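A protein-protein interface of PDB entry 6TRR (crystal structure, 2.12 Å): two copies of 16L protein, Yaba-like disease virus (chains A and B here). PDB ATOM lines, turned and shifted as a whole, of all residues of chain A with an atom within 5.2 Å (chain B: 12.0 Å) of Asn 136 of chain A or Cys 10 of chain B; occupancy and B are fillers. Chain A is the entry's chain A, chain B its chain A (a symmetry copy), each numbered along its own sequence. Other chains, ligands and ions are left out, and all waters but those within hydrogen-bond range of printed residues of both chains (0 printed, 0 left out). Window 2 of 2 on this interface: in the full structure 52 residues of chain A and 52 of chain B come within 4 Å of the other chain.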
ATOM      1  N   ASN A  94      16.128 -17.853   0.546  1.00  0.00           N
ATOM      2  CA  ASN A  94      17.291 -17.986  -0.324  1.00  0.00           C
ATOM      3  C   ASN A  94      17.559 -19.431  -0.727  1.00  0.00           C
ATOM      4  O   ASN A  94      18.694 -19.774  -1.077  1.00  0.00           O
ATOM      5  CB  ASN A  94      18.528 -17.395   0.351  1.00  0.00           C
ATOM      6  CG  ASN A  94      18.955 -18.176   1.572  1.00  0.00           C
ATOM      7  OD1 ASN A  94      18.123 -18.640   2.353  1.00  0.00           O
ATOM      8  ND2 ASN A  94      20.260 -18.336   1.739  1.00  0.00           N
ATOM      9  N   LYS A  99      15.969 -19.711  -5.923  1.00  0.00           N
ATOM     10  CA  LYS A  99      16.921 -19.016  -6.781  1.00  0.00           C
ATOM     11  C   LYS A  99      16.723 -19.402  -8.242  1.00  0.00           C
ATOM     12  O   LYS A  99      16.761 -18.541  -9.129  1.00  0.00           O
ATOM     13  CB  LYS A  99      18.348 -19.321  -6.325  1.00  0.00           C
ATOM     14  CG  LYS A  99      18.710 -18.707  -4.977  1.00  0.00           C
ATOM     15  CD  LYS A  99      20.154 -18.984  -4.606  1.00  0.00           C
ATOM     16  CE  LYS A  99      20.602 -18.121  -3.439  1.00  0.00           C
ATOM     17  NZ  LYS A  99      22.047 -18.302  -3.136  1.00  0.00           N
ATOM     18  N   SER A 134      24.542 -16.285  -6.471  1.00  0.00           N
ATOM     19  CA  SER A 134      25.856 -16.891  -6.307  1.00  0.00           C
ATOM     20  C   SER A 134      26.289 -16.983  -4.851  1.00  0.00           C
ATOM     21  O   SER A 134      27.243 -17.709  -4.557  1.00  0.00           O
ATOM     22  CB  SER A 134      26.907 -16.112  -7.103  1.00  0.00           C
ATOM     23  OG  SER A 134      26.952 -14.750  -6.718  1.00  0.00           O
ATOM     24  N   GLU A 135      25.623 -16.275  -3.941  1.00  0.00           N
ATOM     25  CA  GLU A 135      25.933 -16.404  -2.523  1.00  0.00           C
ATOM     26  C   GLU A 135      25.575 -17.800  -2.031  1.00  0.00           C
ATOM     27  O   GLU A 135      24.661 -18.450  -2.546  1.00  0.00           O
ATOM     28  CB  GLU A 135      25.175 -15.357  -1.705  1.00  0.00           C
ATOM     29  CG  GLU A 135      25.682 -15.170  -0.282  1.00  0.00           C
ATOM     30  CD  GLU A 135      25.009 -13.997   0.406  1.00  0.00           C
ATOM     31  OE1 GLU A 135      25.336 -13.718   1.580  1.00  0.00           O
ATOM     32  OE2 GLU A 135      24.152 -13.351  -0.233  1.00  0.00           O
ATOM     33  N   ASN A 136      26.299 -18.250  -1.012  1.00  0.00           N
ATOM     34  CA  ASN A 136      26.180 -19.611  -0.498  1.00  0.00           C
ATOM     35  C   ASN A 136      26.109 -20.598  -1.658  1.00  0.00           C
ATOM     36  O   ASN A 136      25.137 -21.333  -1.842  1.00  0.00           O
ATOM     37  CB  ASN A 136      24.971 -19.751   0.420  1.00  0.00           C
ATOM     38  CG  ASN A 136      25.051 -18.839   1.624  1.00  0.00           C
ATOM     39  OD1 ASN A 136      25.931 -18.985   2.471  1.00  0.00           O
ATOM     40  ND2 ASN A 136      24.124 -17.892   1.709  1.00  0.00           N
ATOM     41  N   SER A 137      27.178 -20.591  -2.452  1.00  0.00           N
ATOM     42  CA  SER A 137      27.190 -21.340  -3.702  1.00  0.00           C
ATOM     43  C   SER A 137      26.991 -22.833  -3.469  1.00  0.00           C
ATOM     44  O   SER A 137      26.221 -23.479  -4.189  1.00  0.00           O
ATOM     45  CB  SER A 137      28.503 -21.080  -4.439  1.00  0.00           C
ATOM     46  OG  SER A 137      29.604 -21.118  -3.541  1.00  0.00           O
ATOM     47  N   GLU A 138      27.679 -23.401  -2.475  1.00  0.00           N
ATOM     48  CA  GLU A 138      27.626 -24.847  -2.273  1.00  0.00           C
ATOM     49  C   GLU A 138      26.189 -25.345  -2.177  1.00  0.00           C
ATOM     50  O   GLU A 138      25.847 -26.391  -2.742  1.00  0.00           O
ATOM     51  CB  GLU A 138      28.423 -25.239  -1.022  1.00  0.00           C
ATOM     52  CG  GLU A 138      27.824 -24.813   0.324  1.00  0.00           C
ATOM     53  CD  GLU A 138      27.792 -23.306   0.518  1.00  0.00           C
ATOM     54  OE1 GLU A 138      26.784 -22.795   1.056  1.00  0.00           O
ATOM     55  OE2 GLU A 138      28.774 -22.634   0.136  1.00  0.00           O
ATOM     56  N   ASP A 139      25.329 -24.601  -1.478  1.00  0.00           N
ATOM     57  CA  ASP A 139      23.925 -24.984  -1.387  1.00  0.00           C
ATOM     58  C   ASP A 139      23.274 -25.044  -2.763  1.00  0.00           C
ATOM     59  O   ASP A 139      22.412 -25.896  -3.007  1.00  0.00           O
ATOM     60  CB  ASP A 139      23.181 -23.999  -0.480  1.00  0.00           C
ATOM     61  CG  ASP A 139      21.896 -24.576   0.094  1.00  0.00           C
ATOM     62  OD1 ASP A 139      21.592 -25.762  -0.162  1.00  0.00           O
ATOM     63  OD2 ASP A 139      21.190 -23.836   0.811  1.00  0.00           O
ATOM     64  N   LEU A 140      23.682 -24.162  -3.680  1.00  0.00           N
ATOM     65  CA  LEU A 140      23.092 -24.144  -5.013  1.00  0.00           C
ATOM     66  C   LEU A 140      23.670 -25.247  -5.892  1.00  0.00           C
ATOM     67  O   LEU A 140      22.926 -25.955  -6.579  1.00  0.00           O
ATOM     68  CB  LEU A 140      23.301 -22.775  -5.661  1.00  0.00           C
ATOM     69  CG  LEU A 140      22.723 -22.610  -7.070  1.00  0.00           C
ATOM     70  CD1 LEU A 140      21.231 -22.915  -7.098  1.00  0.00           C
ATOM     71  CD2 LEU A 140      22.990 -21.203  -7.585  1.00  0.00           C
ATOM     72  N   CYS B  10      30.490 -14.181   2.504  1.00  0.00           N
ATOM     73  CA  CYS B  10      29.738 -15.363   2.893  1.00  0.00           C
ATOM     74  C   CYS B  10      29.646 -16.357   1.739  1.00  0.00           C
ATOM     75  O   CYS B  10      28.553 -16.720   1.303  1.00  0.00           O
ATOM     76  CB  CYS B  10      28.338 -14.967   3.368  1.00  0.00           C
ATOM     77  SG  CYS B  10      27.435 -16.292   4.204  1.00  0.00           S
ATOM     78  N   ASN B  11      30.807 -16.770   1.229  1.00  0.00           N
ATOM     79  CA  ASN B  11      30.910 -17.897   0.304  1.00  0.00           C
ATOM     80  C   ASN B  11      30.183 -17.592  -1.009  1.00  0.00           C
ATOM     81  O   ASN B  11      29.158 -18.186  -1.350  1.00  0.00           O
ATOM     82  CB  ASN B  11      30.360 -19.175   0.952  1.00  0.00           C
ATOM     83  CG  ASN B  11      30.984 -19.459   2.310  1.00  0.00           C
ATOM     84  OD1 ASN B  11      30.644 -18.824   3.305  1.00  0.00           O
ATOM     85  ND2 ASN B  11      31.898 -20.424   2.355  1.00  0.00           N
ATOM     86  N   PHE B  12      30.749 -16.635  -1.737  1.00  0.00           N
ATOM     87  CA  PHE B  12      30.258 -16.280  -3.061  1.00  0.00           C
ATOM     88  C   PHE B  12      31.040 -17.026  -4.137  1.00  0.00           C
ATOM     89  O   PHE B  12      32.205 -17.386  -3.949  1.00  0.00           O
ATOM     90  CB  PHE B  12      30.367 -14.771  -3.300  1.00  0.00           C
ATOM     91  CG  PHE B  12      29.350 -13.954  -2.544  1.00  0.00           C
ATOM     92  CD1 PHE B  12      28.198 -13.507  -3.166  1.00  0.00           C
ATOM     93  CD2 PHE B  12      29.553 -13.624  -1.213  1.00  0.00           C
ATOM     94  CE1 PHE B  12      27.264 -12.753  -2.477  1.00  0.00           C
ATOM     95  CE2 PHE B  12      28.621 -12.872  -0.519  1.00  0.00           C
ATOM     96  CZ  PHE B  12      27.476 -12.435  -1.155  1.00  0.00           C
ATOM     97  N   ASN B  13      30.381 -17.254  -5.272  1.00  0.00           N
ATOM     98  CA  ASN B  13      30.968 -17.963  -6.409  1.00  0.00           C
ATOM     99  C   ASN B  13      30.674 -17.173  -7.677  1.00  0.00           C
ATOM    100  O   ASN B  13      29.551 -17.208  -8.188  1.00  0.00           O
ATOM    101  CB  ASN B  13      30.411 -19.385  -6.513  1.00  0.00           C
ATOM    102  CG  ASN B  13      31.012 -20.171  -7.665  1.00  0.00           C
ATOM    103  OD1 ASN B  13      31.287 -19.624  -8.732  1.00  0.00           O
ATOM    104  ND2 ASN B  13      31.217 -21.463  -7.452  1.00  0.00           N
ATOM    105  N   ASN B  14      31.687 -16.486  -8.207  1.00  0.00           N
ATOM    106  CA  ASN B  14      31.491 -15.646  -9.382  1.00  0.00           C
ATOM    107  C   ASN B  14      31.347 -16.441 -10.674  1.00  0.00           C
ATOM    108  O   ASN B  14      30.924 -15.868 -11.685  1.00  0.00           O
ATOM    109  CB  ASN B  14      32.646 -14.651  -9.512  1.00  0.00           C
ATOM    110  CG  ASN B  14      32.429 -13.405  -8.677  1.00  0.00           C
ATOM    111  OD1 ASN B  14      32.853 -13.335  -7.523  1.00  0.00           O
ATOM    112  ND2 ASN B  14      31.752 -12.417  -9.253  1.00  0.00           N
ATOM    113  N   SER B  15      31.684 -17.732 -10.676  1.00  0.00           N
ATOM    114  CA  SER B  15      31.366 -18.563 -11.833  1.00  0.00           C
ATOM    115  C   SER B  15      29.856 -18.709 -11.990  1.00  0.00           C
ATOM    116  O   SER B  15      29.325 -18.595 -13.100  1.00  0.00           O
ATOM    117  CB  SER B  15      32.035 -19.930 -11.700  1.00  0.00           C
ATOM    118  OG  SER B  15      33.431 -19.789 -11.501  1.00  0.00           O
ATOM    119  N   ILE B  16      29.148 -18.962 -10.887  1.00  0.00           N
ATOM    120  CA  ILE B  16      27.687 -18.921 -10.907  1.00  0.00           C
ATOM    121  C   ILE B  16      27.215 -17.581 -11.446  1.00  0.00           C
ATOM    122  O   ILE B  16      26.406 -17.511 -12.379  1.00  0.00           O
ATOM    123  CB  ILE B  16      27.124 -19.182  -9.498  1.00  0.00           C
ATOM    124  CG1 ILE B  16      27.332 -20.640  -9.084  1.00  0.00           C
ATOM    125  CG2 ILE B  16      25.638 -18.801  -9.414  1.00  0.00           C
ATOM    126  CD1 ILE B  16      26.325 -21.601  -9.675  1.00  0.00           C
ATOM    127  N   LYS B  17      27.721 -16.494 -10.859  1.00  0.00           N
ATOM    128  CA  LYS B  17      27.282 -15.157 -11.243  1.00  0.00           C
ATOM    129  C   LYS B  17      27.480 -14.924 -12.735  1.00  0.00           C
ATOM    130  O   LYS B  17      26.580 -14.432 -13.423  1.00  0.00           O
ATOM    131  CB  LYS B  17      28.041 -14.109 -10.427  1.00  0.00           C
ATOM    132  CG  LYS B  17      27.581 -12.674 -10.659  1.00  0.00           C
ATOM    133  CD  LYS B  17      28.524 -11.677  -9.995  1.00  0.00           C
ATOM    134  CE  LYS B  17      28.071 -10.236 -10.209  1.00  0.00           C
ATOM    135  NZ  LYS B  17      28.918  -9.258  -9.459  1.00  0.00           N
ATOM    136  N   ILE B  20      24.977 -16.935 -14.842  1.00  0.00           N
ATOM    137  CA  ILE B  20      23.624 -16.386 -14.777  1.00  0.00           C
ATOM    138  C   ILE B  20      23.521 -15.111 -15.606  1.00  0.00           C
ATOM    139  O   ILE B  20      22.543 -14.905 -16.333  1.00  0.00           O
ATOM    140  CB  ILE B  20      23.216 -16.146 -13.312  1.00  0.00           C
ATOM    141  CG1 ILE B  20      23.106 -17.482 -12.574  1.00  0.00           C
ATOM    142  CG2 ILE B  20      21.893 -15.377 -13.233  1.00  0.00           C
ATOM    143  CD1 ILE B  20      22.986 -17.349 -11.085  1.00  0.00           C
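NZ of Lys 99 of chain A lies within hydrogen-bond range of O of Glu 135 of chain A (2.7 Å). The backbone NH (N) of Ser 15 of chain B sits at hydrogen-bond distance from the side-chain amide oxygen (OD1) of Asn 13 of chain B, at 2.7 Å. N of Ile 16 of chain B sits at hydrogen-bond distance from OD1 of Asn 13 of chain B, 3.1 Å away.
Among the printed residues, pairs that only touch across the chains: Ser 134 of chain A with Asn 11 of chain B (3.8 Å), Ser 134 of chain A with Phe 12 of chain B (3.7 Å), Ser 134 of chain A with Ile 16 of chain B (3.7 Å), Ser 134 of chain A with Lys 17 of chain B (3.9 Å), Glu 135 of chain A with Cys 10 of chain B (3.6 Å), Glu 135 of chain A with Asn 11 of chain B (3.7 Å), Glu 135 of chain A with Phe 12 of chain B (3.3 Å), Ser 137 of chain A with Asn 13 of chain B (3.3 Å), Glu 138 of chain A with Asn 11 of chain B (3.9 Å) and Leu 140 of chain A with Ile 16 of chain B (3.96 Å).
Of the 9 printed residues of chain B, 6 touch a printed residue of chain A. Hydrophobic or aromatic side chains of chain B within 4 Å of the printed part of chain A: Phe 12 and Ile 16. Along chain B the printed residues that touch a printed residue of chain A span positions 10 to 17. Among the printed residues, 14 pairs touch across the chains. Among the printed residues, no Asp or Glu carboxylate lies within 4 Å of a Lys or Arg side-chain nitrogen of the other chain.
Of chain B, only Asn 11, Phe 12, Asn 13, Ile 16 and Lys 17 come within 4 Å of Ser 134 of chain A. Of chain B, only Cys 10 and Asn 11 come within 4 Å of Asn 136 of chain A. Of chain B, only Asn 11 and Asn 13 come within 4 Å of Ser 137 of chain A. Glu 138 of chain A touches one residue of chain B. Asp 139 of chain A touches none of the printed residues of chain B. Leu 140 of chain A touches one residue of chain B. Of chain A, only Glu 135 (3.6 Å) and Asn 136 (3.5 Å) come within 4 Å of Cys 10 of chain B. Printed residues of chain A within 4 Å of Asn 11 of chain B: Ser 134, Glu 135, Asn 136, Ser 137 and Glu 138. Printed residues of chain A within 4 Å of Asn 13 of chain B: Ser 134 and Ser 137. The nearest residue of chain B that does not touch Asn 136 of chain A is Phe 12 of chain B (4.8 Å). The nearest printed residue of chain A that does not touch Asn 13 of chain B is Glu 135 of chain A (5.0 Å).
No position is printed for both chains.
The backbone carbonyl oxygen (O) of Asn 11 of chain B sits at hydrogen-bond distance from the backbone NH (N) of Asn 136 of chain A (2.9 Å). The backbone carbonyl oxygen (O) of Ser 134 of chain A lies within hydrogen-bond range of the backbone NH (N) of Asn 13 of chain B. The backbone NH (N) of Ser 137 of chain A lies within hydrogen-bond range of the backbone carbonyl oxygen (O) of Asn 11 of chain B (3.3 Å). The side-chain amide oxygen of Asn 136 of chain A is in hydrogen-bond range of the side-chain sulfur of Cys 10 of chain B (3.5 Å).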
